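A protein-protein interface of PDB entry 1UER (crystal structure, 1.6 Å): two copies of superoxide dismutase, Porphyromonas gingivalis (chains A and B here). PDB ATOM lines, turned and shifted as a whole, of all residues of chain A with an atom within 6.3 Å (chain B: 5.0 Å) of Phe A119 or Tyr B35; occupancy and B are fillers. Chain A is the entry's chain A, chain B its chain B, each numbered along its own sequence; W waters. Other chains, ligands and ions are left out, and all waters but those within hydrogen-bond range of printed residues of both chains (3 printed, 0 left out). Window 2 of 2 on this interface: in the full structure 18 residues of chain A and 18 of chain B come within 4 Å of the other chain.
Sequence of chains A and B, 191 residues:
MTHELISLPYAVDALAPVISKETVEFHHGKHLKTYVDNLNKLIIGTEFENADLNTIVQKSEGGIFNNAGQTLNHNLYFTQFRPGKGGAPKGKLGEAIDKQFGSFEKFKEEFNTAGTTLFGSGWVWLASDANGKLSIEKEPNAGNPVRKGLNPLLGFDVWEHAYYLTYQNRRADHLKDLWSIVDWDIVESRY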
ATOM      1  N   GLY A 115      19.166  11.608   1.352  1.00  0.00           N
ATOM      2  CA  GLY A 115      17.909  10.995   0.949  1.00  0.00           C
ATOM      3  C   GLY A 115      17.531  11.397  -0.451  1.00  0.00           C
ATOM      4  O   GLY A 115      16.956  10.594  -1.216  1.00  0.00           O
ATOM      5  N   THR A 116      17.859  12.633  -0.800  1.00  0.00           N
ATOM      6  CA  THR A 116      17.526  13.154  -2.121  1.00  0.00           C
ATOM      7  C   THR A 116      18.393  12.546  -3.223  1.00  0.00           C
ATOM      8  O   THR A 116      17.865  12.199  -4.295  1.00  0.00           O
ATOM      9  CB  THR A 116      17.630  14.726  -2.148  1.00  0.00           C
ATOM     10  OG1 THR A 116      16.588  15.304  -1.326  1.00  0.00           O
ATOM     11  CG2 THR A 116      17.492  15.236  -3.558  1.00  0.00           C
ATOM     12  N   THR A 117      19.693  12.381  -2.959  1.00  0.00           N
ATOM     13  CA  THR A 117      20.642  11.849  -3.942  1.00  0.00           C
ATOM     14  C   THR A 117      20.701  10.320  -4.075  1.00  0.00           C
ATOM     15  O   THR A 117      21.449   9.777  -4.898  1.00  0.00           O
ATOM     16  CB  THR A 117      22.097  12.368  -3.679  1.00  0.00           C
ATOM     17  OG1 THR A 117      22.599  11.843  -2.444  1.00  0.00           O
ATOM     18  CG2 THR A 117      22.159  13.912  -3.699  1.00  0.00           C
ATOM     19  N   LEU A 118      19.957   9.608  -3.244  1.00  0.00           N
ATOM     20  CA  LEU A 118      19.927   8.143  -3.315  1.00  0.00           C
ATOM     21  C   LEU A 118      19.167   7.803  -4.599  1.00  0.00           C
ATOM     22  O   LEU A 118      17.991   8.108  -4.721  1.00  0.00           O
ATOM     23  CB  LEU A 118      19.171   7.583  -2.095  1.00  0.00           C
ATOM     24  CG  LEU A 118      19.408   6.094  -1.826  1.00  0.00           C
ATOM     25  CD1 LEU A 118      19.016   5.753  -0.366  1.00  0.00           C
ATOM     26  CD2 LEU A 118      18.600   5.255  -2.808  1.00  0.00           C
ATOM     27  N   PHE A 119      19.854   7.198  -5.561  1.00  0.00           N
ATOM     28  CA  PHE A 119      19.236   6.855  -6.837  1.00  0.00           C
ATOM     29  C   PHE A 119      18.452   5.561  -6.785  1.00  0.00           C
ATOM     30  O   PHE A 119      18.994   4.515  -6.411  1.00  0.00           O
ATOM     31  CB  PHE A 119      20.328   6.747  -7.921  1.00  0.00           C
ATOM     32  CG  PHE A 119      19.778   6.692  -9.319  1.00  0.00           C
ATOM     33  CD1 PHE A 119      19.177   7.817  -9.871  1.00  0.00           C
ATOM     34  CD2 PHE A 119      19.848   5.522 -10.066  1.00  0.00           C
ATOM     35  CE1 PHE A 119      18.638   7.795 -11.151  1.00  0.00           C
ATOM     36  CE2 PHE A 119      19.296   5.487 -11.380  1.00  0.00           C
ATOM     37  CZ  PHE A 119      18.696   6.630 -11.906  1.00  0.00           C
ATOM     38  N   GLY A 120      17.186   5.617  -7.207  1.00  0.00           N
ATOM     39  CA  GLY A 120      16.386   4.397  -7.200  1.00  0.00           C
ATOM     40  C   GLY A 120      15.663   4.233  -5.876  1.00  0.00           C
ATOM     41  O   GLY A 120      15.429   5.228  -5.187  1.00  0.00           O
ATOM     42  N   SER A 121      15.318   3.000  -5.512  1.00  0.00           N
ATOM     43  CA  SER A 121      14.612   2.755  -4.238  1.00  0.00           C
ATOM     44  C   SER A 121      15.621   2.569  -3.103  1.00  0.00           C
ATOM     45  O   SER A 121      16.731   2.094  -3.332  1.00  0.00           O
ATOM     46  CB  SER A 121      13.786   1.461  -4.309  1.00  0.00           C
ATOM     47  OG  SER A 121      12.861   1.473  -5.410  1.00  0.00           O
ATOM     48  N   GLY A 122      15.213   2.895  -1.880  1.00  0.00           N
ATOM     49  CA  GLY A 122      16.118   2.697  -0.757  1.00  0.00           C
ATOM     50  C   GLY A 122      15.722   3.469   0.474  1.00  0.00           C
ATOM     51  O   GLY A 122      14.609   4.003   0.544  1.00  0.00           O
ATOM     52  N   LYS A 138      23.369   5.435   3.370  1.00  0.00           N
ATOM     53  CA  LYS A 138      22.434   5.366   2.250  1.00  0.00           C
ATOM     54  C   LYS A 138      22.314   3.875   1.942  1.00  0.00           C
ATOM     55  O   LYS A 138      23.308   3.214   1.604  1.00  0.00           O
ATOM     56  CB  LYS A 138      22.972   6.178   1.057  1.00  0.00           C
ATOM     57  CG  LYS A 138      23.091   7.671   1.406  1.00  0.00           C
ATOM     58  CD  LYS A 138      24.013   8.463   0.447  1.00  0.00           C
ATOM     59  CE  LYS A 138      23.343   8.724  -0.905  1.00  0.00           C
ATOM     60  NZ  LYS A 138      24.242   9.493  -1.872  1.00  0.00           N
ATOM     61  N   PRO A 140      20.652   1.029  -0.390  1.00  0.00           N
ATOM     62  CA  PRO A 140      19.759   0.730  -1.518  1.00  0.00           C
ATOM     63  C   PRO A 140      18.757  -0.378  -1.222  1.00  0.00           C
ATOM     64  O   PRO A 140      19.020  -1.320  -0.449  1.00  0.00           O
ATOM     65  CB  PRO A 140      20.705   0.301  -2.641  1.00  0.00           C
ATOM     66  CG  PRO A 140      22.085   0.805  -2.215  1.00  0.00           C
ATOM     67  CD  PRO A 140      22.060   0.715  -0.693  1.00  0.00           C
ATOM     68  N   GLU A 160       9.574   5.113  -3.892  1.00  0.00           N
ATOM     69  CA  GLU A 160       8.498   6.026  -4.309  1.00  0.00           C
ATOM     70  C   GLU A 160       7.133   5.759  -3.693  1.00  0.00           C
ATOM     71  O   GLU A 160       6.368   6.710  -3.502  1.00  0.00           O
ATOM     72  CB  GLU A 160       8.416   6.094  -5.868  1.00  0.00           C
ATOM     73  CG  GLU A 160       9.653   6.836  -6.434  1.00  0.00           C
ATOM     74  CD  GLU A 160       9.791   6.789  -7.958  1.00  0.00           C
ATOM     75  OE1 GLU A 160       9.541   5.715  -8.583  1.00  0.00           O
ATOM     76  OE2 GLU A 160      10.172   7.849  -8.514  1.00  0.00           O
ATOM     77  N   ARG A 171      10.320  14.378  -3.980  1.00  0.00           N
ATOM     78  CA  ARG A 171      10.897  13.618  -2.870  1.00  0.00           C
ATOM     79  C   ARG A 171      11.526  14.555  -1.819  1.00  0.00           C
ATOM     80  O   ARG A 171      11.377  14.328  -0.625  1.00  0.00           O
ATOM     81  CB  ARG A 171      11.939  12.631  -3.393  1.00  0.00           C
ATOM     82  CG  ARG A 171      12.597  11.786  -2.292  1.00  0.00           C
ATOM     83  CD  ARG A 171      13.890  11.126  -2.763  1.00  0.00           C
ATOM     84  NE  ARG A 171      13.650   9.921  -3.581  1.00  0.00           N
ATOM     85  CZ  ARG A 171      14.629   9.107  -3.934  1.00  0.00           C
ATOM     86  NH1 ARG A 171      15.859   9.411  -3.521  1.00  0.00           N
ATOM     87  NH2 ARG A 171      14.410   8.032  -4.709  1.00  0.00           N
ATOM     88  N   HIS B  31       9.740  13.705 -14.537  1.00  0.00           N
ATOM     89  CA  HIS B  31      10.856  12.771 -14.366  1.00  0.00           C
ATOM     90  C   HIS B  31      11.862  12.789 -15.539  1.00  0.00           C
ATOM     91  O   HIS B  31      13.070  12.921 -15.331  1.00  0.00           O
ATOM     92  CB  HIS B  31      10.338  11.351 -14.165  1.00  0.00           C
ATOM     93  CG  HIS B  31       9.592  11.163 -12.875  1.00  0.00           C
ATOM     94  ND1 HIS B  31      10.208  10.723 -11.721  1.00  0.00           N
ATOM     95  CD2 HIS B  31       8.293  11.372 -12.551  1.00  0.00           C
ATOM     96  CE1 HIS B  31       9.316  10.667 -10.744  1.00  0.00           C
ATOM     97  NE2 HIS B  31       8.148  11.055 -11.220  1.00  0.00           N
ATOM     98  N   LEU B  32      11.363  12.675 -16.767  1.00  0.00           N
ATOM     99  CA  LEU B  32      12.266  12.606 -17.911  1.00  0.00           C
ATOM    100  C   LEU B  32      12.969  13.944 -18.147  1.00  0.00           C
ATOM    101  O   LEU B  32      14.155  13.982 -18.489  1.00  0.00           O
ATOM    102  CB  LEU B  32      11.500  12.126 -19.155  1.00  0.00           C
ATOM    103  CG  LEU B  32      12.309  11.947 -20.448  1.00  0.00           C
ATOM    104  CD1 LEU B  32      13.565  11.113 -20.195  1.00  0.00           C
ATOM    105  CD2 LEU B  32      11.415  11.302 -21.510  1.00  0.00           C
ATOM    106  N   LYS B  33      12.258  15.050 -17.946  1.00  0.00           N
ATOM    107  CA  LYS B  33      12.885  16.356 -18.130  1.00  0.00           C
ATOM    108  C   LYS B  33      14.071  16.447 -17.175  1.00  0.00           C
ATOM    109  O   LYS B  33      15.133  16.955 -17.536  1.00  0.00           O
ATOM    110  CB  LYS B  33      11.889  17.503 -17.855  1.00  0.00           C
ATOM    111  CG  LYS B  33      12.579  18.885 -17.813  1.00  0.00           C
ATOM    112  CD  LYS B  33      11.595  20.017 -17.465  1.00  0.00           C
ATOM    113  CE  LYS B  33      12.080  21.375 -18.015  1.00  0.00           C
ATOM    114  NZ  LYS B  33      13.420  21.762 -17.475  1.00  0.00           N
ATOM    115  N   THR B  34      13.900  15.930 -15.953  1.00  0.00           N
ATOM    116  CA  THR B  34      14.957  15.951 -14.961  1.00  0.00           C
ATOM    117  C   THR B  34      16.150  15.100 -15.403  1.00  0.00           C
ATOM    118  O   THR B  34      17.281  15.531 -15.278  1.00  0.00           O
ATOM    119  CB  THR B  34      14.453  15.446 -13.598  1.00  0.00           C
ATOM    120  OG1 THR B  34      13.534  16.408 -13.074  1.00  0.00           O
ATOM    121  CG2 THR B  34      15.593  15.284 -12.621  1.00  0.00           C
ATOM    122  N   TYR B  35      15.894  13.898 -15.918  1.00  0.00           N
ATOM    123  CA  TYR B  35      16.994  13.039 -16.360  1.00  0.00           C
ATOM    124  C   TYR B  35      17.780  13.721 -17.489  1.00  0.00           C
ATOM    125  O   TYR B  35      18.999  13.673 -17.528  1.00  0.00           O
ATOM    126  CB  TYR B  35      16.459  11.701 -16.880  1.00  0.00           C
ATOM    127  CG  TYR B  35      15.911  10.801 -15.792  1.00  0.00           C
ATOM    128  CD1 TYR B  35      16.666  10.527 -14.642  1.00  0.00           C
ATOM    129  CD2 TYR B  35      14.655  10.198 -15.929  1.00  0.00           C
ATOM    130  CE1 TYR B  35      16.168   9.659 -13.643  1.00  0.00           C
ATOM    131  CE2 TYR B  35      14.157   9.330 -14.938  1.00  0.00           C
ATOM    132  CZ  TYR B  35      14.910   9.070 -13.814  1.00  0.00           C
ATOM    133  OH  TYR B  35      14.408   8.188 -12.870  1.00  0.00           O
ATOM    134  N   VAL B  36      17.060  14.364 -18.397  1.00  0.00           N
ATOM    135  CA  VAL B  36      17.691  15.029 -19.537  1.00  0.00           C
ATOM    136  C   VAL B  36      18.503  16.235 -19.073  1.00  0.00           C
ATOM    137  O   VAL B  36      19.622  16.466 -19.536  1.00  0.00           O
ATOM    138  CB  VAL B  36      16.607  15.479 -20.553  1.00  0.00           C
ATOM    139  CG1 VAL B  36      17.196  16.445 -21.597  1.00  0.00           C
ATOM    140  CG2 VAL B  36      16.014  14.254 -21.233  1.00  0.00           C
ATOM    141  N   ASP B  37      17.931  16.984 -18.140  1.00  0.00           N
ATOM    142  CA  ASP B  37      18.580  18.170 -17.615  1.00  0.00           C
ATOM    143  C   ASP B  37      19.857  17.755 -16.883  1.00  0.00           C
ATOM    144  O   ASP B  37      20.916  18.373 -17.057  1.00  0.00           O
ATOM    145  CB  ASP B  37      17.604  18.907 -16.671  1.00  0.00           C
ATOM    146  CG  ASP B  37      16.521  19.670 -17.418  1.00  0.00           C
ATOM    147  OD1 ASP B  37      16.617  19.809 -18.661  1.00  0.00           O
ATOM    148  OD2 ASP B  37      15.554  20.163 -16.770  1.00  0.00           O
ATOM    149  N   ASN B  38      19.779  16.696 -16.085  1.00  0.00           N
ATOM    150  CA  ASN B  38      20.954  16.233 -15.340  1.00  0.00           C
ATOM    151  C   ASN B  38      22.040  15.692 -16.281  1.00  0.00           C
ATOM    152  O   ASN B  38      23.223  15.920 -16.058  1.00  0.00           O
ATOM    153  CB  ASN B  38      20.571  15.144 -14.333  1.00  0.00           C
ATOM    154  CG  ASN B  38      19.902  15.700 -13.082  1.00  0.00           C
ATOM    155  OD1 ASN B  38      20.024  16.888 -12.766  1.00  0.00           O
ATOM    156  ND2 ASN B  38      19.208  14.823 -12.343  1.00  0.00           N
ATOM    157  N   LEU B  39      21.632  14.932 -17.297  1.00  0.00           N
ATOM    158  CA  LEU B  39      22.588  14.400 -18.262  1.00  0.00           C
ATOM    159  C   LEU B  39      23.373  15.562 -18.885  1.00  0.00           C
ATOM    160  O   LEU B  39      24.597  15.569 -18.866  1.00  0.00           O
ATOM    161  CB  LEU B  39      21.862  13.630 -19.356  1.00  0.00           C
ATOM    162  CG  LEU B  39      22.762  13.112 -20.471  1.00  0.00           C
ATOM    163  CD1 LEU B  39      23.820  12.167 -19.939  1.00  0.00           C
ATOM    164  CD2 LEU B  39      21.876  12.433 -21.481  1.00  0.00           C
ATOM    165  N   ASN B  66      23.518   6.895 -14.896  1.00  0.00           N
ATOM    166  CA  ASN B  66      22.139   6.873 -14.389  1.00  0.00           C
ATOM    167  C   ASN B  66      21.201   7.759 -15.216  1.00  0.00           C
ATOM    168  O   ASN B  66      20.099   7.348 -15.550  1.00  0.00           O
ATOM    169  CB  ASN B  66      22.113   7.292 -12.914  1.00  0.00           C
ATOM    170  CG  ASN B  66      22.718   6.231 -12.018  1.00  0.00           C
ATOM    171  OD1 ASN B  66      22.822   5.071 -12.409  1.00  0.00           O
ATOM    172  ND2 ASN B  66      23.131   6.624 -10.817  1.00  0.00           N
ATOM    173  N   ASN B  67      21.653   8.959 -15.578  1.00  0.00           N
ATOM    174  CA  ASN B  67      20.797   9.833 -16.343  1.00  0.00           C
ATOM    175  C   ASN B  67      20.743   9.488 -17.833  1.00  0.00           C
ATOM    176  O   ASN B  67      19.700   9.660 -18.468  1.00  0.00           O
ATOM    177  CB  ASN B  67      21.233  11.273 -16.107  1.00  0.00           C
ATOM    178  CG  ASN B  67      20.928  11.721 -14.697  1.00  0.00           C
ATOM    179  OD1 ASN B  67      19.769  11.953 -14.361  1.00  0.00           O
ATOM    180  ND2 ASN B  67      21.972  11.842 -13.846  1.00  0.00           N
ATOM    181  N   GLN B  70      18.550   6.329 -18.116  1.00  0.00           N
ATOM    182  CA  GLN B  70      17.135   6.654 -17.977  1.00  0.00           C
ATOM    183  C   GLN B  70      16.602   7.439 -19.179  1.00  0.00           C
ATOM    184  O   GLN B  70      15.445   7.253 -19.597  1.00  0.00           O
ATOM    185  CB  GLN B  70      16.884   7.417 -16.670  1.00  0.00           C
ATOM    186  CG  GLN B  70      16.907   6.511 -15.439  1.00  0.00           C
ATOM    187  CD  GLN B  70      15.737   5.531 -15.438  1.00  0.00           C
ATOM    188  OE1 GLN B  70      15.748   4.535 -16.145  1.00  0.00           O
ATOM    189  NE2 GLN B  70      14.712   5.817 -14.617  1.00  0.00           N
ATOM    190  N   THR B  71      17.420   8.326 -19.737  1.00  0.00           N
ATOM    191  CA  THR B  71      16.978   9.084 -20.902  1.00  0.00           C
ATOM    192  C   THR B  71      16.699   8.115 -22.066  1.00  0.00           C
ATOM    193  O   THR B  71      15.613   8.160 -22.674  1.00  0.00           O
ATOM    194  CB  THR B  71      18.022  10.176 -21.314  1.00  0.00           C
ATOM    195  OG1 THR B  71      18.133  11.162 -20.277  1.00  0.00           O
ATOM    196  CG2 THR B  71      17.573  10.893 -22.581  1.00  0.00           C
ATOM    197  N   HIS B  74      13.488   5.848 -21.373  1.00  0.00           N
ATOM    198  CA  HIS B  74      12.223   6.552 -21.528  1.00  0.00           C
ATOM    199  C   HIS B  74      11.953   6.952 -22.978  1.00  0.00           C
ATOM    200  O   HIS B  74      10.800   6.921 -23.409  1.00  0.00           O
ATOM    201  CB  HIS B  74      12.176   7.781 -20.596  1.00  0.00           C
ATOM    202  CG  HIS B  74      12.011   7.416 -19.149  1.00  0.00           C
ATOM    203  ND1 HIS B  74      13.084   7.201 -18.313  1.00  0.00           N
ATOM    204  CD2 HIS B  74      10.900   7.219 -18.393  1.00  0.00           C
ATOM    205  CE1 HIS B  74      12.642   6.890 -17.102  1.00  0.00           C
ATOM    206  NE2 HIS B  74      11.323   6.895 -17.128  1.00  0.00           N
ATOM    207  N   ASN B 141      17.458  -0.300 -11.704  1.00  0.00           N
ATOM    208  CA  ASN B 141      17.559   1.145 -11.797  1.00  0.00           C
ATOM    209  C   ASN B 141      17.604   1.687 -13.217  1.00  0.00           C
ATOM    210  O   ASN B 141      16.602   1.588 -13.916  1.00  0.00           O
ATOM    211  CB  ASN B 141      18.753   1.607 -10.918  1.00  0.00           C
ATOM    212  CG  ASN B 141      18.498   1.334  -9.411  1.00  0.00           C
ATOM    213  OD1 ASN B 141      17.370   1.026  -9.027  1.00  0.00           O
ATOM    214  ND2 ASN B 141      19.558   1.428  -8.567  1.00  0.00           N
ATOM    215  N   ALA B 142      18.728   2.241 -13.661  1.00  0.00           N
ATOM    216  CA  ALA B 142      18.799   2.825 -15.002  1.00  0.00           C
ATOM    217  C   ALA B 142      19.315   1.917 -16.106  1.00  0.00           C
ATOM    218  O   ALA B 142      19.580   2.414 -17.219  1.00  0.00           O
ATOM    219  CB  ALA B 142      19.654   4.106 -14.968  1.00  0.00           C
ATOM    220  N   TRP B 159       9.768   1.107 -12.270  1.00  0.00           N
ATOM    221  CA  TRP B 159       9.981   2.100 -11.235  1.00  0.00           C
ATOM    222  C   TRP B 159       8.536   2.398 -10.777  1.00  0.00           C
ATOM    223  O   TRP B 159       7.604   2.486 -11.604  1.00  0.00           O
ATOM    224  CB  TRP B 159      10.578   3.374 -11.825  1.00  0.00           C
ATOM    225  CG  TRP B 159      12.041   3.294 -12.002  1.00  0.00           C
ATOM    226  CD1 TRP B 159      12.717   2.458 -12.842  1.00  0.00           C
ATOM    227  CD2 TRP B 159      13.029   4.125 -11.367  1.00  0.00           C
ATOM    228  NE1 TRP B 159      14.080   2.727 -12.771  1.00  0.00           N
ATOM    229  CE2 TRP B 159      14.292   3.742 -11.877  1.00  0.00           C
ATOM    230  CE3 TRP B 159      12.967   5.157 -10.419  1.00  0.00           C
ATOM    231  CZ2 TRP B 159      15.494   4.358 -11.469  1.00  0.00           C
ATOM    232  CZ3 TRP B 159      14.161   5.769 -10.007  1.00  0.00           C
ATOM    233  CH2 TRP B 159      15.404   5.373 -10.532  1.00  0.00           C
ATOM    234  N   HIS B 161       7.068   5.136  -9.950  1.00  0.00           N
ATOM    235  CA  HIS B 161       6.444   6.323 -10.564  1.00  0.00           C
ATOM    236  C   HIS B 161       5.727   6.015 -11.880  1.00  0.00           C
ATOM    237  O   HIS B 161       4.883   6.807 -12.301  1.00  0.00           O
ATOM    238  CB  HIS B 161       7.449   7.468 -10.771  1.00  0.00           C
ATOM    239  CG  HIS B 161       8.596   7.140 -11.689  1.00  0.00           C
ATOM    240  ND1 HIS B 161       9.911   7.225 -11.284  1.00  0.00           N
ATOM    241  CD2 HIS B 161       8.626   6.786 -12.997  1.00  0.00           C
ATOM    242  CE1 HIS B 161      10.707   6.947 -12.309  1.00  0.00           C
ATOM    243  NE2 HIS B 161       9.953   6.676 -13.356  1.00  0.00           N
HETATM  244  O   HOH W   1      12.241   9.122 -10.015  1.00  0.00           O
HETATM  245  O   HOH W   2      18.521   1.903  -5.356  1.00  0.00           O
HETATM  246  O   HOH W   3      15.859   0.455  -6.824  1.00  0.00           O
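ND1 of His B161 lies within hydrogen-bond range of OE2 of Glu A160, 2.9 Å away.
A ring nitrogen (ND1) of His B74 lies within hydrogen-bond range of the backbone carbonyl oxygen (O) of Gln B70, at 2.7 Å.
OH of Tyr B35 sits at hydrogen-bond distance from NE2 of Gln B70 (3.0 Å).
The backbone carbonyl oxygen (O) of Gly A120 lies within hydrogen-bond range of the guanidinium group (NH2) of Arg A171.
The backbone carbonyl oxygen of Asn B141 lies within hydrogen-bond range of the indole nitrogen of Trp B159 (3.0 Å).
Of the 12 printed residues of chain A, 3 touch a printed residue of chain B.
Hydrophobic or aromatic side chains of chain A that line the printed part of chain B: Phe A119.
Of the 18 printed residues of chain B, 8 touch a printed residue of chain A.
Printed residues of chain B that touch a printed residue of chain A: His B31, Tyr B35, Asn B66, Gln B70, Asn B141, Ala B142, Trp B159 and His B161.
Hydrophobic or aromatic side chains of chain B within 4 Å of the printed part of chain A: His B31, Tyr B35, Ala B142, Trp B159 and His B161.
Along chain B the printed residues that touch a printed residue of chain A span positions 31 to 161.
Among the printed residues, 11 pairs touch across the chains.
Phe A119 touches just these residues of chain B: Tyr B35 (3.97 Å), Asn B66 (3.5 Å), Gln B70 (3.96 Å), Asn B141 (3.8 Å), Ala B142 (3.9 Å) and Trp B159 (3.8 Å).
Of chain A, only Phe A119 (3.97 Å) comes within 4 Å of Tyr B35.
Of the printed residues of chain A, Asn B141 touches Phe A119 (3.8 Å) and Gly A120 (3.96 Å).
Of the printed residues of chain A, Asn B66 touches Phe A119 (3.5 Å).
Of the printed residues of chain A, Gln B70 touches Phe A119.
Of the printed residues of chain A, His B161 touches Glu A160 (2.9 Å).
Lys B33 touches none of the printed residues of chain A.
The nearest printed residue of chain B that does not touch Phe A119 is Asn B67 (5.3 Å).
The nearest residue of chain A that does not touch Tyr B35 is Glu A160 (6.1 Å).
No position is printed for both chains.
Water W2 lies within hydrogen-bond range of the backbone carbonyl oxygen (O) of Ser A121 (2.7 Å), the backbone carbonyl oxygen (O) of Phe A119 (2.9 Å) and the side-chain amide nitrogen (ND2) of Asn B141 (3.4 Å).
Water W3 bridges OD1 of Asn B141 and N of Ser A121.
Water W1 lies within hydrogen-bond range of the side-chain carboxylate of Glu A160, a ring nitrogen (ND1) of His B31 and a ring nitrogen (ND1) of His B161.
Among the printed residues, pairs that only touch across the chains: Phe A119 with Tyr B35, Phe A119 with Asn B66, Phe A119 with Gln B70, Phe A119 with Asn B141, Phe A119 with Ala B142, Phe A119 with Trp B159, Gly A120 with Asn B141, Gly A120 with Trp B159, Glu A160 with His B31 and Glu A160 with Trp B159.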
